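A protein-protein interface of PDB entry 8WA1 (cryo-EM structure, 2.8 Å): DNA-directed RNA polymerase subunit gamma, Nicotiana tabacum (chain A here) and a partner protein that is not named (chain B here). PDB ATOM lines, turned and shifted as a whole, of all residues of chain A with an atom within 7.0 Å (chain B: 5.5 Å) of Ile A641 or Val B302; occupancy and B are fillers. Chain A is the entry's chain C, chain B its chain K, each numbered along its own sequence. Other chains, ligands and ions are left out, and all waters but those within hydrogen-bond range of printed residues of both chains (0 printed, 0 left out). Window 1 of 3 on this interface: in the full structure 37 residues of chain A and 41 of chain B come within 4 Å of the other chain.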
ATOM      1  N   PRO A 564      18.117   6.296 -10.885  1.00  0.00           N
ATOM      2  CA  PRO A 564      17.889   7.712 -11.213  1.00  0.00           C
ATOM      3  C   PRO A 564      17.808   7.998 -12.705  1.00  0.00           C
ATOM      4  O   PRO A 564      17.632   9.166 -13.079  1.00  0.00           O
ATOM      5  CB  PRO A 564      19.099   8.419 -10.584  1.00  0.00           C
ATOM      6  CG  PRO A 564      19.588   7.473  -9.531  1.00  0.00           C
ATOM      7  CD  PRO A 564      19.335   6.104 -10.081  1.00  0.00           C
ATOM      8  N   TRP A 611      27.424  20.201  -1.938  1.00  0.00           N
ATOM      9  CA  TRP A 611      28.430  20.779  -2.819  1.00  0.00           C
ATOM     10  C   TRP A 611      29.073  21.973  -2.127  1.00  0.00           C
ATOM     11  O   TRP A 611      28.369  22.827  -1.577  1.00  0.00           O
ATOM     12  CB  TRP A 611      27.819  21.207  -4.158  1.00  0.00           C
ATOM     13  CG  TRP A 611      27.343  20.064  -5.004  1.00  0.00           C
ATOM     14  CD1 TRP A 611      26.110  19.482  -4.976  1.00  0.00           C
ATOM     15  CD2 TRP A 611      28.090  19.372  -6.014  1.00  0.00           C
ATOM     16  NE1 TRP A 611      26.044  18.468  -5.899  1.00  0.00           N
ATOM     17  CE2 TRP A 611      27.246  18.380  -6.550  1.00  0.00           C
ATOM     18  CE3 TRP A 611      29.390  19.493  -6.513  1.00  0.00           C
ATOM     19  CZ2 TRP A 611      27.660  17.514  -7.561  1.00  0.00           C
ATOM     20  CZ3 TRP A 611      29.799  18.633  -7.517  1.00  0.00           C
ATOM     21  CH2 TRP A 611      28.937  17.657  -8.031  1.00  0.00           C
ATOM     22  N   THR A 626      38.886   9.764 -15.582  1.00  0.00           N
ATOM     23  CA  THR A 626      38.424  10.786 -16.503  1.00  0.00           C
ATOM     24  C   THR A 626      37.014  11.239 -16.124  1.00  0.00           C
ATOM     25  O   THR A 626      36.304  10.541 -15.397  1.00  0.00           O
ATOM     26  CB  THR A 626      38.444  10.256 -17.934  1.00  0.00           C
ATOM     27  OG1 THR A 626      37.594   9.106 -18.033  1.00  0.00           O
ATOM     28  CG2 THR A 626      39.858   9.872 -18.340  1.00  0.00           C
ATOM     29  N   PRO A 627      36.594  12.418 -16.590  1.00  0.00           N
ATOM     30  CA  PRO A 627      35.224  12.868 -16.312  1.00  0.00           C
ATOM     31  C   PRO A 627      34.193  11.877 -16.827  1.00  0.00           C
ATOM     32  O   PRO A 627      34.292  11.371 -17.948  1.00  0.00           O
ATOM     33  CB  PRO A 627      35.134  14.206 -17.050  1.00  0.00           C
ATOM     34  CG  PRO A 627      36.531  14.687 -17.121  1.00  0.00           C
ATOM     35  CD  PRO A 627      37.389  13.464 -17.257  1.00  0.00           C
ATOM     36  N   ILE A 628      33.192  11.601 -15.988  1.00  0.00           N
ATOM     37  CA  ILE A 628      32.145  10.657 -16.366  1.00  0.00           C
ATOM     38  C   ILE A 628      31.258  11.249 -17.453  1.00  0.00           C
ATOM     39  O   ILE A 628      30.707  10.523 -18.289  1.00  0.00           O
ATOM     40  CB  ILE A 628      31.333  10.242 -15.126  1.00  0.00           C
ATOM     41  CG1 ILE A 628      30.744  11.471 -14.434  1.00  0.00           C
ATOM     42  CG2 ILE A 628      32.209   9.466 -14.156  1.00  0.00           C
ATOM     43  CD1 ILE A 628      29.952  11.147 -13.188  1.00  0.00           C
ATOM     44  N   GLU A 629      31.113  12.571 -17.465  1.00  0.00           N
ATOM     45  CA  GLU A 629      30.295  13.248 -18.460  1.00  0.00           C
ATOM     46  C   GLU A 629      30.764  14.690 -18.577  1.00  0.00           C
ATOM     47  O   GLU A 629      31.096  15.332 -17.577  1.00  0.00           O
ATOM     48  CB  GLU A 629      28.806  13.194 -18.097  1.00  0.00           C
ATOM     49  CG  GLU A 629      27.868  13.270 -19.290  1.00  0.00           C
ATOM     50  CD  GLU A 629      26.413  13.084 -18.905  1.00  0.00           C
ATOM     51  OE1 GLU A 629      25.794  14.056 -18.423  1.00  0.00           O
ATOM     52  OE2 GLU A 629      25.890  11.963 -19.077  1.00  0.00           O
ATOM     53  N   VAL A 630      30.788  15.194 -19.809  1.00  0.00           N
ATOM     54  CA  VAL A 630      31.225  16.554 -20.100  1.00  0.00           C
ATOM     55  C   VAL A 630      30.156  17.231 -20.943  1.00  0.00           C
ATOM     56  O   VAL A 630      29.773  16.714 -21.998  1.00  0.00           O
ATOM     57  CB  VAL A 630      32.583  16.581 -20.829  1.00  0.00           C
ATOM     58  CG1 VAL A 630      32.966  18.010 -21.181  1.00  0.00           C
ATOM     59  CG2 VAL A 630      33.662  15.934 -19.978  1.00  0.00           C
ATOM     60  N   HIS A 631      29.677  18.382 -20.482  1.00  0.00           N
ATOM     61  CA  HIS A 631      28.652  19.149 -21.178  1.00  0.00           C
ATOM     62  C   HIS A 631      29.283  20.390 -21.793  1.00  0.00           C
ATOM     63  O   HIS A 631      29.836  21.228 -21.076  1.00  0.00           O
ATOM     64  CB  HIS A 631      27.523  19.546 -20.225  1.00  0.00           C
ATOM     65  CG  HIS A 631      26.757  18.384 -19.679  1.00  0.00           C
ATOM     66  ND1 HIS A 631      25.760  18.526 -18.738  1.00  0.00           N
ATOM     67  CD2 HIS A 631      26.839  17.058 -19.943  1.00  0.00           C
ATOM     68  CE1 HIS A 631      25.262  17.338 -18.445  1.00  0.00           C
ATOM     69  NE2 HIS A 631      25.899  16.430 -19.163  1.00  0.00           N
ATOM     70  N   TYR A 639      31.169  22.149 -19.075  1.00  0.00           N
ATOM     71  CA  TYR A 639      31.097  21.636 -17.714  1.00  0.00           C
ATOM     72  C   TYR A 639      31.705  20.242 -17.671  1.00  0.00           C
ATOM     73  O   TYR A 639      31.308  19.362 -18.443  1.00  0.00           O
ATOM     74  CB  TYR A 639      29.649  21.593 -17.222  1.00  0.00           C
ATOM     75  CG  TYR A 639      28.881  22.881 -17.420  1.00  0.00           C
ATOM     76  CD1 TYR A 639      28.180  23.118 -18.594  1.00  0.00           C
ATOM     77  CD2 TYR A 639      28.849  23.853 -16.429  1.00  0.00           C
ATOM     78  CE1 TYR A 639      27.473  24.290 -18.779  1.00  0.00           C
ATOM     79  CE2 TYR A 639      28.143  25.029 -16.606  1.00  0.00           C
ATOM     80  CZ  TYR A 639      27.459  25.242 -17.783  1.00  0.00           C
ATOM     81  OH  TYR A 639      26.755  26.410 -17.964  1.00  0.00           O
ATOM     82  N   GLU A 640      32.664  20.041 -16.772  1.00  0.00           N
ATOM     83  CA  GLU A 640      33.329  18.755 -16.605  1.00  0.00           C
ATOM     84  C   GLU A 640      32.898  18.151 -15.279  1.00  0.00           C
ATOM     85  O   GLU A 640      33.266  18.659 -14.214  1.00  0.00           O
ATOM     86  CB  GLU A 640      34.850  18.908 -16.665  1.00  0.00           C
ATOM     87  CG  GLU A 640      35.375  19.355 -18.021  1.00  0.00           C
ATOM     88  CD  GLU A 640      36.886  19.487 -18.046  1.00  0.00           C
ATOM     89  OE1 GLU A 640      37.519  19.294 -16.986  1.00  0.00           O
ATOM     90  OE2 GLU A 640      37.443  19.784 -19.124  1.00  0.00           O
ATOM     91  N   ILE A 641      32.125  17.073 -15.343  1.00  0.00           N
ATOM     92  CA  ILE A 641      31.614  16.393 -14.160  1.00  0.00           C
ATOM     93  C   ILE A 641      32.545  15.234 -13.838  1.00  0.00           C
ATOM     94  O   ILE A 641      32.738  14.333 -14.663  1.00  0.00           O
ATOM     95  CB  ILE A 641      30.174  15.897 -14.365  1.00  0.00           C
ATOM     96  CG1 ILE A 641      29.214  17.073 -14.561  1.00  0.00           C
ATOM     97  CG2 ILE A 641      29.736  15.042 -13.186  1.00  0.00           C
ATOM     98  CD1 ILE A 641      28.993  17.463 -16.007  1.00  0.00           C
ATOM     99  N   TYR A 642      33.114  15.251 -12.638  1.00  0.00           N
ATOM    100  CA  TYR A 642      33.985  14.191 -12.159  1.00  0.00           C
ATOM    101  C   TYR A 642      33.253  13.371 -11.105  1.00  0.00           C
ATOM    102  O   TYR A 642      32.068  13.576 -10.833  1.00  0.00           O
ATOM    103  CB  TYR A 642      35.288  14.757 -11.584  1.00  0.00           C
ATOM    104  CG  TYR A 642      36.224  15.335 -12.621  1.00  0.00           C
ATOM    105  CD1 TYR A 642      36.026  16.611 -13.130  1.00  0.00           C
ATOM    106  CD2 TYR A 642      37.312  14.607 -13.082  1.00  0.00           C
ATOM    107  CE1 TYR A 642      36.881  17.145 -14.074  1.00  0.00           C
ATOM    108  CE2 TYR A 642      38.174  15.133 -14.027  1.00  0.00           C
ATOM    109  CZ  TYR A 642      37.955  16.402 -14.519  1.00  0.00           C
ATOM    110  OH  TYR A 642      38.810  16.927 -15.460  1.00  0.00           O
ATOM    111  N   GLY A 643      33.981  12.424 -10.515  1.00  0.00           N
ATOM    112  CA  GLY A 643      33.379  11.568  -9.506  1.00  0.00           C
ATOM    113  C   GLY A 643      32.988  12.319  -8.248  1.00  0.00           C
ATOM    114  O   GLY A 643      31.903  12.109  -7.700  1.00  0.00           O
ATOM    115  N   HIS A 644      33.859  13.210  -7.775  1.00  0.00           N
ATOM    116  CA  HIS A 644      33.663  13.880  -6.496  1.00  0.00           C
ATOM    117  C   HIS A 644      33.692  15.401  -6.601  1.00  0.00           C
ATOM    118  O   HIS A 644      33.657  16.078  -5.566  1.00  0.00           O
ATOM    119  CB  HIS A 644      34.716  13.412  -5.490  1.00  0.00           C
ATOM    120  CG  HIS A 644      34.704  11.936  -5.245  1.00  0.00           C
ATOM    121  ND1 HIS A 644      33.943  11.352  -4.255  1.00  0.00           N
ATOM    122  CD2 HIS A 644      35.364  10.924  -5.857  1.00  0.00           C
ATOM    123  CE1 HIS A 644      34.132  10.045  -4.270  1.00  0.00           C
ATOM    124  NE2 HIS A 644      34.990   9.759  -5.233  1.00  0.00           N
ATOM    125  N   TYR A 645      33.757  15.961  -7.806  1.00  0.00           N
ATOM    126  CA  TYR A 645      33.817  17.411  -7.937  1.00  0.00           C
ATOM    127  C   TYR A 645      33.384  17.826  -9.335  1.00  0.00           C
ATOM    128  O   TYR A 645      33.425  17.038 -10.283  1.00  0.00           O
ATOM    129  CB  TYR A 645      35.219  17.946  -7.628  1.00  0.00           C
ATOM    130  CG  TYR A 645      36.338  17.196  -8.313  1.00  0.00           C
ATOM    131  CD1 TYR A 645      36.938  16.101  -7.704  1.00  0.00           C
ATOM    132  CD2 TYR A 645      36.800  17.585  -9.562  1.00  0.00           C
ATOM    133  CE1 TYR A 645      37.962  15.412  -8.322  1.00  0.00           C
ATOM    134  CE2 TYR A 645      37.824  16.903 -10.187  1.00  0.00           C
ATOM    135  CZ  TYR A 645      38.401  15.816  -9.565  1.00  0.00           C
ATOM    136  OH  TYR A 645      39.422  15.133 -10.186  1.00  0.00           O
ATOM    137  N   LEU A 646      32.968  19.087  -9.441  1.00  0.00           N
ATOM    138  CA  LEU A 646      32.548  19.699 -10.695  1.00  0.00           C
ATOM    139  C   LEU A 646      33.429  20.908 -10.974  1.00  0.00           C
ATOM    140  O   LEU A 646      33.618  21.757 -10.097  1.00  0.00           O
ATOM    141  CB  LEU A 646      31.076  20.118 -10.635  1.00  0.00           C
ATOM    142  CG  LEU A 646      30.555  20.955 -11.804  1.00  0.00           C
ATOM    143  CD1 LEU A 646      30.566  20.149 -13.092  1.00  0.00           C
ATOM    144  CD2 LEU A 646      29.160  21.483 -11.507  1.00  0.00           C
ATOM    145  N   ILE A 647      33.963  20.985 -12.188  1.00  0.00           N
ATOM    146  CA  ILE A 647      34.908  22.033 -12.572  1.00  0.00           C
ATOM    147  C   ILE A 647      34.344  22.710 -13.817  1.00  0.00           C
ATOM    148  O   ILE A 647      34.437  22.187 -14.930  1.00  0.00           O
ATOM    149  CB  ILE A 647      36.315  21.487 -12.817  1.00  0.00           C
ATOM    150  CG1 ILE A 647      36.866  20.860 -11.536  1.00  0.00           C
ATOM    151  CG2 ILE A 647      37.237  22.590 -13.310  1.00  0.00           C
ATOM    152  CD1 ILE A 647      38.243  20.268 -11.691  1.00  0.00           C
ATOM    153  N   ASP B 297      21.178  16.713 -17.916  1.00  0.00           N
ATOM    154  CA  ASP B 297      21.144  16.136 -16.580  1.00  0.00           C
ATOM    155  C   ASP B 297      22.140  16.855 -15.681  1.00  0.00           C
ATOM    156  O   ASP B 297      23.282  17.106 -16.079  1.00  0.00           O
ATOM    157  CB  ASP B 297      21.464  14.639 -16.616  1.00  0.00           C
ATOM    158  CG  ASP B 297      20.458  13.846 -17.426  1.00  0.00           C
ATOM    159  OD1 ASP B 297      19.490  14.452 -17.933  1.00  0.00           O
ATOM    160  OD2 ASP B 297      20.635  12.617 -17.555  1.00  0.00           O
ATOM    161  N   ASP B 298      21.702  17.186 -14.465  1.00  0.00           N
ATOM    162  CA  ASP B 298      22.585  17.812 -13.497  1.00  0.00           C
ATOM    163  C   ASP B 298      23.679  16.831 -13.077  1.00  0.00           C
ATOM    164  O   ASP B 298      23.510  15.614 -13.189  1.00  0.00           O
ATOM    165  CB  ASP B 298      21.789  18.283 -12.280  1.00  0.00           C
ATOM    166  CG  ASP B 298      20.797  17.247 -11.794  1.00  0.00           C
ATOM    167  OD1 ASP B 298      20.150  16.602 -12.644  1.00  0.00           O
ATOM    168  OD2 ASP B 298      20.665  17.078 -10.564  1.00  0.00           O
ATOM    169  N   PRO B 299      24.824  17.343 -12.606  1.00  0.00           N
ATOM    170  CA  PRO B 299      25.916  16.435 -12.208  1.00  0.00           C
ATOM    171  C   PRO B 299      25.504  15.421 -11.155  1.00  0.00           C
ATOM    172  O   PRO B 299      25.959  14.269 -11.191  1.00  0.00           O
ATOM    173  CB  PRO B 299      26.989  17.398 -11.680  1.00  0.00           C
ATOM    174  CG  PRO B 299      26.710  18.687 -12.371  1.00  0.00           C
ATOM    175  CD  PRO B 299      25.220  18.759 -12.512  1.00  0.00           C
ATOM    176  N   THR B 300      24.649  15.823 -10.212  1.00  0.00           N
ATOM    177  CA  THR B 300      24.169  14.890  -9.202  1.00  0.00           C
ATOM    178  C   THR B 300      23.458  13.707  -9.843  1.00  0.00           C
ATOM    179  O   THR B 300      23.620  12.563  -9.402  1.00  0.00           O
ATOM    180  CB  THR B 300      23.236  15.607  -8.228  1.00  0.00           C
ATOM    181  OG1 THR B 300      22.029  15.973  -8.906  1.00  0.00           O
ATOM    182  CG2 THR B 300      23.898  16.861  -7.702  1.00  0.00           C
ATOM    183  N   THR B 301      22.690  13.959 -10.905  1.00  0.00           N
ATOM    184  CA  THR B 301      21.934  12.886 -11.544  1.00  0.00           C
ATOM    185  C   THR B 301      22.858  11.848 -12.167  1.00  0.00           C
ATOM    186  O   THR B 301      22.678  10.644 -11.955  1.00  0.00           O
ATOM    187  CB  THR B 301      20.990  13.463 -12.598  1.00  0.00           C
ATOM    188  OG1 THR B 301      20.027  14.312 -11.963  1.00  0.00           O
ATOM    189  CG2 THR B 301      20.264  12.346 -13.331  1.00  0.00           C
ATOM    190  N   VAL B 302      23.859  12.289 -12.934  1.00  0.00           N
ATOM    191  CA  VAL B 302      24.745  11.335 -13.598  1.00  0.00           C
ATOM    192  C   VAL B 302      25.631  10.628 -12.579  1.00  0.00           C
ATOM    193  O   VAL B 302      25.928   9.432 -12.717  1.00  0.00           O
ATOM    194  CB  VAL B 302      25.571  12.034 -14.695  1.00  0.00           C
ATOM    195  CG1 VAL B 302      24.667  12.487 -15.827  1.00  0.00           C
ATOM    196  CG2 VAL B 302      26.342  13.213 -14.129  1.00  0.00           C
ATOM    197  N   ILE B 303      26.052  11.343 -11.533  1.00  0.00           N
ATOM    198  CA  ILE B 303      26.845  10.708 -10.485  1.00  0.00           C
ATOM    199  C   ILE B 303      26.037   9.614  -9.797  1.00  0.00           C
ATOM    200  O   ILE B 303      26.529   8.496  -9.591  1.00  0.00           O
ATOM    201  CB  ILE B 303      27.351  11.760  -9.482  1.00  0.00           C
ATOM    202  CG1 ILE B 303      28.430  12.633 -10.125  1.00  0.00           C
ATOM    203  CG2 ILE B 303      27.887  11.091  -8.228  1.00  0.00           C
ATOM    204  CD1 ILE B 303      28.928  13.747  -9.230  1.00  0.00           C
ATOM    205  N   GLU B 304      24.781   9.908  -9.449  1.00  0.00           N
ATOM    206  CA  GLU B 304      23.940   8.907  -8.805  1.00  0.00           C
ATOM    207  C   GLU B 304      23.644   7.747  -9.744  1.00  0.00           C
ATOM    208  O   GLU B 304      23.589   6.594  -9.312  1.00  0.00           O
ATOM    209  CB  GLU B 304      22.641   9.547  -8.314  1.00  0.00           C
ATOM    210  CG  GLU B 304      22.812  10.462  -7.114  1.00  0.00           C
ATOM    211  CD  GLU B 304      21.510  11.107  -6.685  1.00  0.00           C
ATOM    212  OE1 GLU B 304      20.491  10.909  -7.378  1.00  0.00           O
ATOM    213  OE2 GLU B 304      21.503  11.813  -5.654  1.00  0.00           O
ATOM    214  N   LYS B 305      23.461   8.029 -11.037  1.00  0.00           N
ATOM    215  CA  LYS B 305      23.221   6.960 -12.001  1.00  0.00           C
ATOM    216  C   LYS B 305      24.402   6.001 -12.070  1.00  0.00           C
ATOM    217  O   LYS B 305      24.226   4.777 -11.993  1.00  0.00           O
ATOM    218  CB  LYS B 305      22.936   7.552 -13.381  1.00  0.00           C
ATOM    219  CG  LYS B 305      21.524   8.081 -13.560  1.00  0.00           C
ATOM    220  CD  LYS B 305      21.388   8.852 -14.863  1.00  0.00           C
ATOM    221  CE  LYS B 305      21.971   8.078 -16.036  1.00  0.00           C
ATOM    222  NZ  LYS B 305      21.342   6.740 -16.199  1.00  0.00           N
ATOM    223  N   GLU B 306      25.616   6.538 -12.215  1.00  0.00           N
ATOM    224  CA  GLU B 306      26.787   5.671 -12.314  1.00  0.00           C
ATOM    225  C   GLU B 306      27.030   4.920 -11.010  1.00  0.00           C
ATOM    226  O   GLU B 306      27.363   3.725 -11.027  1.00  0.00           O
ATOM    227  CB  GLU B 306      28.014   6.489 -12.714  1.00  0.00           C
ATOM    228  CG  GLU B 306      29.201   5.646 -13.150  1.00  0.00           C
ATOM    229  CD  GLU B 306      30.102   6.373 -14.127  1.00  0.00           C
ATOM    230  OE1 GLU B 306      29.725   7.480 -14.563  1.00  0.00           O
ATOM    231  OE2 GLU B 306      31.179   5.838 -14.460  1.00  0.00           O
ATOM    232  N   GLU B 307      26.864   5.598  -9.869  1.00  0.00           N
ATOM    233  CA  GLU B 307      27.020   4.925  -8.584  1.00  0.00           C
ATOM    234  C   GLU B 307      26.006   3.801  -8.421  1.00  0.00           C
ATOM    235  O   GLU B 307      26.350   2.711  -7.953  1.00  0.00           O
ATOM    236  CB  GLU B 307      26.889   5.935  -7.443  1.00  0.00           C
ATOM    237  CG  GLU B 307      28.106   6.827  -7.253  1.00  0.00           C
ATOM    238  CD  GLU B 307      29.294   6.079  -6.677  1.00  0.00           C
ATOM    239  OE1 GLU B 307      29.089   4.997  -6.085  1.00  0.00           O
ATOM    240  OE2 GLU B 307      30.433   6.572  -6.815  1.00  0.00           O
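Of chain B, only Pro B299 (3.7 Å) and Val B302 (3.97 Å) come within 4 Å of Ile A641. Of chain A, only Glu A629 (3.2 Å) and Ile A641 (3.97 Å) come within 4 Å of Val B302. Of the printed residues of chain A, Ile B303 touches Ile A628 (3.7 Å), Tyr A642 (3.5 Å) and Gly A643 (3.7 Å). Printed residues of chain A within 4 Å of Glu B306: Ile A628 (3.2 Å). His A644 touches none of the printed residues of chain B. The nearest residue of chain A that does not touch Val B302 is Ile A628 (4.3 Å). The nearest printed residue of chain B that does not touch Pro A564 is Thr B301 (4.1 Å).
Of the 11 printed residues of chain B, 8 touch a printed residue of chain A. Of the 17 printed residues of chain A, 9 touch a printed residue of chain B. Hydrophobic or aromatic side chains of chain A within 4 Å of the printed part of chain B: Pro A564, Trp A611, Ile A628, His A631, Ile A641 and Leu A646. Along chain A the printed residues that touch a printed residue of chain B span positions 564 to 646. Among the printed residues, 12 pairs touch across the chains.
Among the printed residues, pairs that only touch across the chains: His A631 with Asp B297 (3.1 Å), Ile A628 with Glu B306 (3.2 Å), Trp A611 with Thr B300 (3.2 Å), Glu A629 with Val B302 (3.2 Å), Tyr A642 with Ile B303 (3.5 Å), Ile A641 with Pro B299 (3.7 Å), Gly A643 with Ile B303 (3.7 Å), Ile A628 with Ile B303 (3.7 Å), Pro A564 with Lys B305 (3.8 Å), Leu A646 with Pro B299 (3.8 Å), Pro A564 with Glu B304 (3.9 Å) and Ile A641 with Val B302 (3.97 Å).
OG1 of Thr B300 is in hydrogen-bond range of OD2 of Asp B298, 2.4 Å away. O of Ile A641 lies within hydrogen-bond range of N of Ile A628 (3.1 Å). NE2 of His A631 sits at hydrogen-bond distance from OE1 of Glu A629, at 2.5 Å. The backbone NH (N) of Ile A641 sits at hydrogen-bond distance from the backbone carbonyl oxygen (O) of Glu A629 (3.0 Å). The backbone NH of Tyr A639 is in hydrogen-bond range of the backbone carbonyl oxygen of His A631, 2.6 Å away. The side-chain hydroxyl (OH) of Tyr A642 sits at hydrogen-bond distance from the side-chain carboxylate (OE1) of Glu A640 (3.1 Å).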
